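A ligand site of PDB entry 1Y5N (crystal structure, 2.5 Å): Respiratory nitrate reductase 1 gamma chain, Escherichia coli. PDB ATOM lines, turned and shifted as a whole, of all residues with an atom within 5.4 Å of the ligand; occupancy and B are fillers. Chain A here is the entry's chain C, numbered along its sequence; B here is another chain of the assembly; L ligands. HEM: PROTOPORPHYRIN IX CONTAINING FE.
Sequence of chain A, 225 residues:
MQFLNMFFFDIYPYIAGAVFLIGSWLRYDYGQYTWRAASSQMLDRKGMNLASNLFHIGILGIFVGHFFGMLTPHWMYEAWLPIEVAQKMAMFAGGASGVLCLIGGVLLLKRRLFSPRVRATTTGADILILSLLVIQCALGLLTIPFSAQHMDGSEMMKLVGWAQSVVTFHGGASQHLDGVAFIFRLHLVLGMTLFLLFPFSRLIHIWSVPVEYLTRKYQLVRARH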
ATOM      1  N   ALA A  37       6.324  30.320   9.345  1.00  0.00           N
ATOM      2  CA  ALA A  37       6.179  29.100  10.132  1.00  0.00           C
ATOM      3  C   ALA A  37       5.702  27.910   9.321  1.00  0.00           C
ATOM      4  O   ALA A  37       5.843  26.760   9.761  1.00  0.00           O
ATOM      5  CB  ALA A  37       5.222  29.358  11.273  1.00  0.00           C
ATOM      6  N   ALA A  38       5.128  28.167   8.146  1.00  0.00           N
ATOM      7  CA  ALA A  38       4.632  27.117   7.281  1.00  0.00           C
ATOM      8  C   ALA A  38       3.550  26.268   7.928  1.00  0.00           C
ATOM      9  O   ALA A  38       3.717  25.061   8.079  1.00  0.00           O
ATOM     10  CB  ALA A  38       5.790  26.205   6.843  1.00  0.00           C
ATOM     11  N   SER A  39       2.430  26.885   8.315  1.00  0.00           N
ATOM     12  CA  SER A  39       1.368  26.123   8.945  1.00  0.00           C
ATOM     13  C   SER A  39       0.850  25.058   8.000  1.00  0.00           C
ATOM     14  O   SER A  39       0.922  25.223   6.789  1.00  0.00           O
ATOM     15  CB  SER A  39       0.215  27.030   9.359  1.00  0.00           C
ATOM     16  OG  SER A  39      -0.910  26.254   9.768  1.00  0.00           O
ATOM     17  N   SER A  40       0.302  23.987   8.561  1.00  0.00           N
ATOM     18  CA  SER A  40      -0.237  22.868   7.776  1.00  0.00           C
ATOM     19  C   SER A  40      -1.564  22.466   8.388  1.00  0.00           C
ATOM     20  O   SER A  40      -2.211  21.514   7.947  1.00  0.00           O
ATOM     21  CB  SER A  40       0.728  21.670   7.822  1.00  0.00           C
ATOM     22  OG  SER A  40       0.854  21.155   9.141  1.00  0.00           O
ATOM     23  N   GLN A  41      -1.970  23.208   9.405  1.00  0.00           N
ATOM     24  CA  GLN A  41      -3.198  22.959  10.140  1.00  0.00           C
ATOM     25  C   GLN A  41      -4.453  22.960   9.258  1.00  0.00           C
ATOM     26  O   GLN A  41      -5.290  22.067   9.367  1.00  0.00           O
ATOM     27  CB  GLN A  41      -3.324  24.017  11.232  1.00  0.00           C
ATOM     28  CG  GLN A  41      -4.125  23.622  12.447  1.00  0.00           C
ATOM     29  CD  GLN A  41      -4.379  24.810  13.359  1.00  0.00           C
ATOM     30  OE1 GLN A  41      -3.529  25.690  13.490  1.00  0.00           O
ATOM     31  NE2 GLN A  41      -5.547  24.838  13.988  1.00  0.00           N
ATOM     32  N   MET A  48      -4.242  18.258  15.722  1.00  0.00           N
ATOM     33  CA  MET A  48      -3.236  19.321  15.765  1.00  0.00           C
ATOM     34  C   MET A  48      -3.167  20.120  17.051  1.00  0.00           C
ATOM     35  O   MET A  48      -2.088  20.532  17.469  1.00  0.00           O
ATOM     36  CB  MET A  48      -3.405  20.259  14.572  1.00  0.00           C
ATOM     37  CG  MET A  48      -2.619  19.839  13.362  1.00  0.00           C
ATOM     38  SD  MET A  48      -0.842  19.770  13.701  1.00  0.00           S
ATOM     39  CE  MET A  48      -0.367  21.409  13.244  1.00  0.00           C
ATOM     40  N   SER A  52       0.550  19.828  18.552  1.00  0.00           N
ATOM     41  CA  SER A  52       1.390  21.006  18.492  1.00  0.00           C
ATOM     42  C   SER A  52       1.624  21.693  19.838  1.00  0.00           C
ATOM     43  O   SER A  52       2.704  22.230  20.094  1.00  0.00           O
ATOM     44  CB  SER A  52       0.833  22.022  17.495  1.00  0.00           C
ATOM     45  OG  SER A  52       1.754  23.073  17.295  1.00  0.00           O
ATOM     46  N   PHE A  55       4.057  19.372  21.823  1.00  0.00           N
ATOM     47  CA  PHE A  55       5.388  19.592  21.275  1.00  0.00           C
ATOM     48  C   PHE A  55       5.999  20.933  21.633  1.00  0.00           C
ATOM     49  O   PHE A  55       7.102  20.988  22.210  1.00  0.00           O
ATOM     50  CB  PHE A  55       5.368  19.445  19.752  1.00  0.00           C
ATOM     51  CG  PHE A  55       6.705  19.675  19.096  1.00  0.00           C
ATOM     52  CD1 PHE A  55       7.156  20.968  18.836  1.00  0.00           C
ATOM     53  CD2 PHE A  55       7.534  18.610  18.786  1.00  0.00           C
ATOM     54  CE1 PHE A  55       8.417  21.198  18.273  1.00  0.00           C
ATOM     55  CE2 PHE A  55       8.796  18.819  18.224  1.00  0.00           C
ATOM     56  CZ  PHE A  55       9.237  20.124  17.968  1.00  0.00           C
ATOM     57  N   HIS A  56       5.310  22.021  21.304  1.00  0.00           N
ATOM     58  CA  HIS A  56       5.836  23.356  21.577  1.00  0.00           C
ATOM     59  C   HIS A  56       6.004  23.708  23.049  1.00  0.00           C
ATOM     60  O   HIS A  56       7.048  24.255  23.440  1.00  0.00           O
ATOM     61  CB  HIS A  56       5.000  24.436  20.871  1.00  0.00           C
ATOM     62  CG  HIS A  56       5.341  24.609  19.420  1.00  0.00           C
ATOM     63  ND1 HIS A  56       4.695  23.904  18.425  1.00  0.00           N
ATOM     64  CD2 HIS A  56       6.288  25.343  18.800  1.00  0.00           C
ATOM     65  CE1 HIS A  56       5.239  24.186  17.256  1.00  0.00           C
ATOM     66  NE2 HIS A  56       6.213  25.058  17.455  1.00  0.00           N
ATOM     67  N   ILE A  59       9.065  21.563  24.213  1.00  0.00           N
ATOM     68  CA  ILE A  59      10.309  22.043  23.622  1.00  0.00           C
ATOM     69  C   ILE A  59      10.716  23.408  24.203  1.00  0.00           C
ATOM     70  O   ILE A  59      11.899  23.737  24.252  1.00  0.00           O
ATOM     71  CB  ILE A  59      10.168  22.186  22.094  1.00  0.00           C
ATOM     72  CG1 ILE A  59      11.536  22.361  21.452  1.00  0.00           C
ATOM     73  CG2 ILE A  59       9.292  23.377  21.754  1.00  0.00           C
ATOM     74  CD1 ILE A  59      12.280  21.064  21.298  1.00  0.00           C
ATOM     75  N   LEU A  60       9.730  24.192  24.608  1.00  0.00           N
ATOM     76  CA  LEU A  60      10.015  25.505  25.176  1.00  0.00           C
ATOM     77  C   LEU A  60      10.539  25.367  26.593  1.00  0.00           C
ATOM     78  O   LEU A  60      11.398  26.145  27.010  1.00  0.00           O
ATOM     79  CB  LEU A  60       8.753  26.388  25.166  1.00  0.00           C
ATOM     80  CG  LEU A  60       8.335  26.937  23.796  1.00  0.00           C
ATOM     81  CD1 LEU A  60       6.967  27.566  23.890  1.00  0.00           C
ATOM     82  CD2 LEU A  60       9.367  27.953  23.308  1.00  0.00           C
ATOM     83  N   LEU A 108       3.208  14.568  15.689  1.00  0.00           N
ATOM     84  CA  LEU A 108       3.341  15.427  14.511  1.00  0.00           C
ATOM     85  C   LEU A 108       4.038  14.713  13.350  1.00  0.00           C
ATOM     86  O   LEU A 108       3.730  14.956  12.187  1.00  0.00           O
ATOM     87  CB  LEU A 108       4.142  16.687  14.844  1.00  0.00           C
ATOM     88  CG  LEU A 108       3.510  17.718  15.763  1.00  0.00           C
ATOM     89  CD1 LEU A 108       4.529  18.795  16.062  1.00  0.00           C
ATOM     90  CD2 LEU A 108       2.255  18.298  15.130  1.00  0.00           C
ATOM     91  N   ARG A 111       1.732  12.274  11.667  1.00  0.00           N
ATOM     92  CA  ARG A 111       0.826  13.074  10.845  1.00  0.00           C
ATOM     93  C   ARG A 111       1.427  13.468   9.513  1.00  0.00           C
ATOM     94  O   ARG A 111       0.844  13.262   8.456  1.00  0.00           O
ATOM     95  CB  ARG A 111       0.414  14.323  11.615  1.00  0.00           C
ATOM     96  CG  ARG A 111      -0.436  15.291  10.831  1.00  0.00           C
ATOM     97  CD  ARG A 111      -1.080  16.304  11.752  1.00  0.00           C
ATOM     98  NE  ARG A 111      -1.812  17.334  11.020  1.00  0.00           N
ATOM     99  CZ  ARG A 111      -1.255  18.307  10.320  1.00  0.00           C
ATOM    100  NH1 ARG A 111      -2.026  19.185   9.695  1.00  0.00           N
ATOM    101  NH2 ARG A 111       0.063  18.425  10.250  1.00  0.00           N
ATOM    102  N   ARG A 112       2.621  14.059   9.574  1.00  0.00           N
ATOM    103  CA  ARG A 112       3.355  14.530   8.410  1.00  0.00           C
ATOM    104  C   ARG A 112       3.715  13.435   7.426  1.00  0.00           C
ATOM    105  O   ARG A 112       3.938  13.682   6.244  1.00  0.00           O
ATOM    106  CB  ARG A 112       4.626  15.231   8.855  1.00  0.00           C
ATOM    107  CG  ARG A 112       5.463  15.826   7.731  1.00  0.00           C
ATOM    108  CD  ARG A 112       6.362  16.912   8.266  1.00  0.00           C
ATOM    109  NE  ARG A 112       5.577  18.053   8.711  1.00  0.00           N
ATOM    110  CZ  ARG A 112       4.931  18.846   7.880  1.00  0.00           C
ATOM    111  NH1 ARG A 112       4.980  18.614   6.577  1.00  0.00           N
ATOM    112  NH2 ARG A 112       4.240  19.883   8.341  1.00  0.00           N
ATOM    113  N   ASP A 126      11.275  19.572   5.924  1.00  0.00           N
ATOM    114  CA  ASP A 126      10.344  19.508   7.042  1.00  0.00           C
ATOM    115  C   ASP A 126      10.319  18.139   7.729  1.00  0.00           C
ATOM    116  O   ASP A 126      10.092  18.059   8.931  1.00  0.00           O
ATOM    117  CB  ASP A 126       8.924  19.880   6.584  1.00  0.00           C
ATOM    118  CG  ASP A 126       8.870  21.227   5.888  1.00  0.00           C
ATOM    119  OD1 ASP A 126       9.480  22.201   6.394  1.00  0.00           O
ATOM    120  OD2 ASP A 126       8.205  21.323   4.824  1.00  0.00           O
ATOM    121  N   ILE A 129      14.201  17.846   9.554  1.00  0.00           N
ATOM    122  CA  ILE A 129      14.241  18.588  10.806  1.00  0.00           C
ATOM    123  C   ILE A 129      13.332  18.058  11.918  1.00  0.00           C
ATOM    124  O   ILE A 129      13.724  18.021  13.079  1.00  0.00           O
ATOM    125  CB  ILE A 129      13.937  20.097  10.550  1.00  0.00           C
ATOM    126  CG1 ILE A 129      15.171  20.935  10.895  1.00  0.00           C
ATOM    127  CG2 ILE A 129      12.755  20.565  11.363  1.00  0.00           C
ATOM    128  CD1 ILE A 129      16.362  20.675   9.990  1.00  0.00           C
ATOM    129  N   LEU A 130      12.115  17.667  11.576  1.00  0.00           N
ATOM    130  CA  LEU A 130      11.200  17.160  12.583  1.00  0.00           C
ATOM    131  C   LEU A 130      11.731  15.858  13.138  1.00  0.00           C
ATOM    132  O   LEU A 130      11.693  15.620  14.350  1.00  0.00           O
ATOM    133  CB  LEU A 130       9.806  16.920  12.000  1.00  0.00           C
ATOM    134  CG  LEU A 130       8.852  16.334  13.049  1.00  0.00           C
ATOM    135  CD1 LEU A 130       8.588  17.387  14.127  1.00  0.00           C
ATOM    136  CD2 LEU A 130       7.560  15.858  12.383  1.00  0.00           C
ATOM    137  N   LEU A 133      14.788  16.359  15.516  1.00  0.00           N
ATOM    138  CA  LEU A 133      14.318  16.870  16.808  1.00  0.00           C
ATOM    139  C   LEU A 133      13.751  15.734  17.658  1.00  0.00           C
ATOM    140  O   LEU A 133      14.105  15.595  18.832  1.00  0.00           O
ATOM    141  CB  LEU A 133      13.257  17.959  16.630  1.00  0.00           C
ATOM    142  CG  LEU A 133      13.729  19.361  16.211  1.00  0.00           C
ATOM    143  CD1 LEU A 133      12.517  20.239  16.039  1.00  0.00           C
ATOM    144  CD2 LEU A 133      14.643  19.962  17.258  1.00  0.00           C
ATOM    145  N   ARG A 202      12.625  25.258   8.365  1.00  0.00           N
ATOM    146  CA  ARG A 202      11.504  26.041   8.846  1.00  0.00           C
ATOM    147  C   ARG A 202      11.785  26.647  10.206  1.00  0.00           C
ATOM    148  O   ARG A 202      11.091  27.589  10.631  1.00  0.00           O
ATOM    149  CB  ARG A 202      10.261  25.158   8.931  1.00  0.00           C
ATOM    150  CG  ARG A 202      10.352  24.068   9.980  1.00  0.00           C
ATOM    151  CD  ARG A 202       9.178  23.132   9.873  1.00  0.00           C
ATOM    152  NE  ARG A 202       7.908  23.838   9.987  1.00  0.00           N
ATOM    153  CZ  ARG A 202       6.744  23.338   9.576  1.00  0.00           C
ATOM    154  NH1 ARG A 202       6.696  22.137   9.013  1.00  0.00           N
ATOM    155  NH2 ARG A 202       5.633  24.030   9.750  1.00  0.00           N
ATOM    156  N   LEU A 203      12.809  26.128  10.895  1.00  0.00           N
ATOM    157  CA  LEU A 203      13.168  26.606  12.226  1.00  0.00           C
ATOM    158  C   LEU A 203      13.324  28.125  12.336  1.00  0.00           C
ATOM    159  O   LEU A 203      13.240  28.675  13.438  1.00  0.00           O
ATOM    160  CB  LEU A 203      14.445  25.924  12.719  1.00  0.00           C
ATOM    161  CG  LEU A 203      14.346  24.407  12.938  1.00  0.00           C
ATOM    162  CD1 LEU A 203      15.561  23.945  13.709  1.00  0.00           C
ATOM    163  CD2 LEU A 203      13.085  24.049  13.705  1.00  0.00           C
ATOM    164  N   HIS A 205      11.291  30.249  11.951  1.00  0.00           N
ATOM    165  CA  HIS A 205      10.116  30.873  12.568  1.00  0.00           C
ATOM    166  C   HIS A 205      10.417  31.304  13.993  1.00  0.00           C
ATOM    167  O   HIS A 205       9.866  32.288  14.480  1.00  0.00           O
ATOM    168  CB  HIS A 205       8.839  29.987  12.518  1.00  0.00           C
ATOM    169  CG  HIS A 205       8.863  28.764  13.391  1.00  0.00           C
ATOM    170  ND1 HIS A 205       9.632  27.654  13.102  1.00  0.00           N
ATOM    171  CD2 HIS A 205       8.079  28.406  14.440  1.00  0.00           C
ATOM    172  CE1 HIS A 205       9.319  26.677  13.935  1.00  0.00           C
ATOM    173  NE2 HIS A 205       8.375  27.105  14.758  1.00  0.00           N
ATOM    174  N   ILE A 206      11.326  30.579  14.639  1.00  0.00           N
ATOM    175  CA  ILE A 206      11.706  30.889  16.009  1.00  0.00           C
ATOM    176  C   ILE A 206      12.174  32.337  16.173  1.00  0.00           C
ATOM    177  O   ILE A 206      11.735  33.044  17.082  1.00  0.00           O
ATOM    178  CB  ILE A 206      12.799  29.921  16.497  1.00  0.00           C
ATOM    179  CG1 ILE A 206      12.308  28.471  16.324  1.00  0.00           C
ATOM    180  CG2 ILE A 206      13.111  30.178  17.952  1.00  0.00           C
ATOM    181  CD1 ILE A 206      13.370  27.430  16.621  1.00  0.00           C
ATOM    182  N   VAL A 209       9.277  34.870  16.919  1.00  0.00           N
ATOM    183  CA  VAL A 209       8.321  34.822  18.041  1.00  0.00           C
ATOM    184  C   VAL A 209       7.794  36.255  18.310  1.00  0.00           C
ATOM    185  O   VAL A 209       8.534  37.144  18.742  1.00  0.00           O
ATOM    186  CB  VAL A 209       8.995  34.203  19.295  1.00  0.00           C
ATOM    187  CG1 VAL A 209      10.330  34.864  19.575  1.00  0.00           C
ATOM    188  CG2 VAL A 209       8.079  34.349  20.485  1.00  0.00           C
ATOM    189  N   PRO A 210       6.498  36.471  18.052  1.00  0.00           N
ATOM    190  CA  PRO A 210       5.712  37.718  18.190  1.00  0.00           C
ATOM    191  C   PRO A 210       5.571  38.383  19.554  1.00  0.00           C
ATOM    192  O   PRO A 210       4.462  38.667  20.003  1.00  0.00           O
ATOM    193  CB  PRO A 210       4.352  37.311  17.631  1.00  0.00           C
ATOM    194  CG  PRO A 210       4.228  35.922  18.117  1.00  0.00           C
ATOM    195  CD  PRO A 210       5.591  35.339  17.807  1.00  0.00           C
ATOM    196  N   ILE B  88      -1.390  30.435  19.486  1.00  0.00           N
ATOM    197  CA  ILE B  88      -0.532  30.383  18.315  1.00  0.00           C
ATOM    198  C   ILE B  88       0.025  29.049  17.841  1.00  0.00           C
ATOM    199  O   ILE B  88       0.236  28.873  16.649  1.00  0.00           O
ATOM    200  CB  ILE B  88       0.631  31.383  18.470  1.00  0.00           C
ATOM    201  CG1 ILE B  88       1.254  31.662  17.111  1.00  0.00           C
ATOM    202  CG2 ILE B  88       1.660  30.838  19.447  1.00  0.00           C
ATOM    203  CD1 ILE B  88       1.872  33.048  17.010  1.00  0.00           C
ATOM    204  N   PHE B  89       0.261  28.108  18.747  1.00  0.00           N
ATOM    205  CA  PHE B  89       0.794  26.819  18.323  1.00  0.00           C
ATOM    206  C   PHE B  89      -0.251  26.051  17.532  1.00  0.00           C
ATOM    207  O   PHE B  89       0.068  25.109  16.815  1.00  0.00           O
ATOM    208  CB  PHE B  89       1.234  25.987  19.512  1.00  0.00           C
ATOM    209  CG  PHE B  89       2.252  26.659  20.353  1.00  0.00           C
ATOM    210  CD1 PHE B  89       3.357  27.256  19.771  1.00  0.00           C
ATOM    211  CD2 PHE B  89       2.112  26.705  21.738  1.00  0.00           C
ATOM    212  CE1 PHE B  89       4.323  27.904  20.560  1.00  0.00           C
ATOM    213  CE2 PHE B  89       3.076  27.339  22.537  1.00  0.00           C
ATOM    214  CZ  PHE B  89       4.182  27.940  21.941  1.00  0.00           C
ATOM    215  N   ALA B  90      -1.508  26.464  17.683  1.00  0.00           N
ATOM    216  CA  ALA B  90      -2.633  25.840  16.978  1.00  0.00           C
ATOM    217  C   ALA B  90      -3.873  26.695  17.145  1.00  0.00           C
ATOM    218  O   ALA B  90      -4.409  26.829  18.247  1.00  0.00           O
ATOM    219  CB  ALA B  90      -2.883  24.432  17.520  1.00  0.00           C
ATOM    220  N   GLY B 219       3.082  33.997   8.689  1.00  0.00           N
ATOM    221  CA  GLY B 219       2.201  32.844   8.667  1.00  0.00           C
ATOM    222  C   GLY B 219       1.698  32.337  10.005  1.00  0.00           C
ATOM    223  O   GLY B 219       1.544  31.123  10.158  1.00  0.00           O
ATOM    224  N   TRP B 220       1.413  33.231  10.954  1.00  0.00           N
ATOM    225  CA  TRP B 220       0.895  32.822  12.269  1.00  0.00           C
ATOM    226  C   TRP B 220      -0.569  32.419  12.160  1.00  0.00           C
ATOM    227  O   TRP B 220      -1.163  31.868  13.090  1.00  0.00           O
ATOM    228  CB  TRP B 220       1.033  33.956  13.289  1.00  0.00           C
ATOM    229  CG  TRP B 220       2.438  34.393  13.540  1.00  0.00           C
ATOM    230  CD1 TRP B 220       2.924  35.674  13.499  1.00  0.00           C
ATOM    231  CD2 TRP B 220       3.563  33.561  13.842  1.00  0.00           C
ATOM    232  NE1 TRP B 220       4.269  35.696  13.749  1.00  0.00           N
ATOM    233  CE2 TRP B 220       4.688  34.408  13.964  1.00  0.00           C
ATOM    234  CE3 TRP B 220       3.721  32.184  14.030  1.00  0.00           C
ATOM    235  CZ2 TRP B 220       5.965  33.914  14.270  1.00  0.00           C
ATOM    236  CZ3 TRP B 220       5.007  31.699  14.331  1.00  0.00           C
ATOM    237  CH2 TRP B 220       6.106  32.557  14.441  1.00  0.00           C
ATOM    238  N   ARG B 221      -1.131  32.696  10.984  1.00  0.00           N
ATOM    239  CA  ARG B 221      -2.521  32.401  10.643  1.00  0.00           C
ATOM    240  C   ARG B 221      -3.615  32.647  11.687  1.00  0.00           C
ATOM    241  O   ARG B 221      -4.570  31.869  11.798  1.00  0.00           O
ATOM    242  CB  ARG B 221      -2.638  30.965  10.094  1.00  0.00           C
ATOM    243  CG  ARG B 221      -1.957  29.888  10.914  1.00  0.00           C
ATOM    244  CD  ARG B 221      -2.947  29.196  11.848  1.00  0.00           C
ATOM    245  NE  ARG B 221      -2.326  28.172  12.682  1.00  0.00           N
ATOM    246  CZ  ARG B 221      -1.453  28.421  13.650  1.00  0.00           C
ATOM    247  NH1 ARG B 221      -1.100  29.668  13.927  1.00  0.00           N
ATOM    248  NH2 ARG B 221      -0.942  27.414  14.345  1.00  0.00           N
HETATM  249  CHA HEM L   1       5.660  24.490  13.689  1.00  0.00           C
HETATM  250  CHB HEM L   1       4.907  28.577  16.156  1.00  0.00           C
HETATM  251  CHC HEM L   1       9.007  27.683  18.604  1.00  0.00           C
HETATM  252  CHD HEM L   1       9.769  23.637  16.135  1.00  0.00           C
HETATM  253  C1A HEM L   1       5.085  25.659  14.119  1.00  0.00           C
HETATM  254  C2A HEM L   1       3.851  26.273  13.637  1.00  0.00           C
HETATM  255  C3A HEM L   1       3.637  27.395  14.316  1.00  0.00           C
HETATM  256  C4A HEM L   1       4.747  27.539  15.260  1.00  0.00           C
HETATM  257  CMA HEM L   1       2.458  28.430  14.200  1.00  0.00           C
HETATM  258  CAA HEM L   1       2.975  25.664  12.516  1.00  0.00           C
HETATM  259  CBA HEM L   1       1.782  24.816  13.108  1.00  0.00           C
HETATM  260  CGA HEM L   1       0.622  24.522  12.132  1.00  0.00           C
HETATM  261  O1A HEM L   1      -0.402  25.286  12.212  1.00  0.00           O
HETATM  262  O2A HEM L   1       0.802  23.559  11.315  1.00  0.00           O
HETATM  263  C1B HEM L   1       5.967  28.707  17.049  1.00  0.00           C
HETATM  264  C2B HEM L   1       6.163  29.822  18.013  1.00  0.00           C
HETATM  265  C3B HEM L   1       7.321  29.563  18.696  1.00  0.00           C
HETATM  266  C4B HEM L   1       7.855  28.296  18.161  1.00  0.00           C
HETATM  267  CMB HEM L   1       5.171  31.027  18.139  1.00  0.00           C
HETATM  268  CAB HEM L   1       8.040  30.400  19.830  1.00  0.00           C
HETATM  269  CBB HEM L   1       7.433  30.950  20.930  1.00  0.00           C
HETATM  270  C1C HEM L   1       9.585  26.527  18.162  1.00  0.00           C
HETATM  271  C2C HEM L   1      10.830  25.924  18.670  1.00  0.00           C
HETATM  272  C3C HEM L   1      11.039  24.788  17.972  1.00  0.00           C
HETATM  273  C4C HEM L   1       9.927  24.665  17.027  1.00  0.00           C
HETATM  274  CMC HEM L   1      11.710  26.548  19.811  1.00  0.00           C
HETATM  275  CAC HEM L   1      12.204  23.756  18.089  1.00  0.00           C
HETATM  276  CBC HEM L   1      13.317  23.947  17.318  1.00  0.00           C
HETATM  277  C1D HEM L   1       8.723  23.504  15.241  1.00  0.00           C
HETATM  278  C2D HEM L   1       8.572  22.394  14.294  1.00  0.00           C
HETATM  279  C3D HEM L   1       7.426  22.637  13.621  1.00  0.00           C
HETATM  280  C4D HEM L   1       6.847  23.898  14.139  1.00  0.00           C
HETATM  281  CMD HEM L   1       9.566  21.201  14.128  1.00  0.00           C
HETATM  282  CAD HEM L   1       6.687  21.837  12.484  1.00  0.00           C
HETATM  283  CBD HEM L   1       5.798  20.632  12.948  1.00  0.00           C
HETATM  284  CGD HEM L   1       5.194  19.897  11.739  1.00  0.00           C
HETATM  285  O1D HEM L   1       4.029  20.287  11.368  1.00  0.00           O
HETATM  286  O2D HEM L   1       5.939  18.966  11.237  1.00  0.00           O
HETATM  287  NA  HEM L   1       5.622  26.457  15.109  1.00  0.00           N
HETATM  288  NB  HEM L   1       7.017  27.798  17.171  1.00  0.00           N
HETATM  289  NC  HEM L   1       9.041  25.733  17.166  1.00  0.00           N
HETATM  290  ND  HEM L   1       7.657  24.407  15.117  1.00  0.00           N
HETATM  291 FE   HEM L   1       7.290  26.090  16.116  1.00  0.00          FE
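NH1 of Arg 202 is in salt-bridge range of O2D of the ligand (3.9 Å). A ring nitrogen (NE2) of His 205 is bound to an iron atom (FE) of the ligand, at 2.0 Å. The backbone NH (N) of Ser 40 is in hydrogen-bond range of an oxygen (O2A) of the ligand. O1A of the ligand sits at hydrogen-bond distance from OG of Ser 39 (2.7 Å). The side-chain amide oxygen (OE1) of Gln 41 sits close to an oxygen (O1A) of the ligand (3.4 Å). O2D of the ligand lies within salt-bridge range of NE of Arg 112 (2.7 Å). The side-chain hydroxyl (OG) of Ser 40 lies within hydrogen-bond range of an oxygen (O2A) of the ligand, at 3.2 Å. An oxygen (O1A) of the ligand is in salt-bridge range of the guanidinium group (NH2) of Arg 221 of chain B (3.1 Å). O2A of the ligand is in hydrogen-bond range of N of Gln 41, 3.4 Å away. A ring nitrogen (NE2) of His 56 is bound to an iron atom (FE) of the ligand (2.0 Å).
Ala 37 touches the ligand (CB to C3A, 3.95 Å). Met 48 touches the ligand (CE to O2A, 3.1 Å). Phe 55 touches the ligand. CG1 of Ile 59 touches CAC of the ligand (3.7 Å). Leu 108 touches the ligand (CD1 to CBD, 3.8 Å). Leu 130 touches the ligand. Leu 133 touches the ligand. CD2 of Leu 203 touches CBC of the ligand, 3.6 Å away. Ile 206 touches the ligand. Val 209 touches the ligand. Ile 88 of chain B touches the ligand (O to CMA, 3.3 Å). Phe 89 of chain B touches the ligand (CE1 to C2B, 3.7 Å). Trp 220 of chain B touches the ligand. Hydrophobic or aromatic side chains within 4 Å of the ligand: Ala 37, Met 48, Phe 55, His 56, Ile 59, Leu 108, Leu 130, Leu 133, Leu 203, His 205, Ile 206, Val 209, Ile 88 of chain B, Phe 89 of chain B and Trp 220 of chain B. Within 4 Å of the ligand: Ala 37, Ser 39, Ser 40, Gln 41, Met 48, Phe 55, His 56, Ile 59, Leu 108, Arg 112, Leu 130, Leu 133, Arg 202, Leu 203, His 205, Ile 206, Val 209, Ile 88 of chain B, Phe 89 of chain B, Trp 220 of chain B and Arg 221 of chain B. Along chain A the residues within 4 Å of the ligand span positions 37 to 209. The nearest printed residue that does not touch the ligand is Ile 129 (4.3 Å).
The guanidinium group (NH2) of Arg 221 of chain B is in hydrogen-bond range of the backbone carbonyl oxygen (O) of Ile 88 of chain B (3.0 Å). NE of Arg 221 of chain B sits at hydrogen-bond distance from OE1 of Gln 41, 2.9 Å away. OD1 of Asp 126 is in salt-bridge range of NH1 of Arg 202 (3.8 Å). The backbone carbonyl oxygen of Ala 38 is in hydrogen-bond range of the guanidinium group of Arg 202, 2.7 Å away. The side-chain hydroxyl (OG) of Ser 52 lies within hydrogen-bond range of the backbone carbonyl oxygen (O) of Phe 89 of chain B (2.7 Å). O of Ser 52 is in hydrogen-bond range of ND1 of His 56, at 3.1 Å. The side-chain sulfur of Met 48 lies close to the guanidinium group of Arg 111. O of Ser 40 lies within hydrogen-bond range of NH1 of Arg 111, at 2.9 Å.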
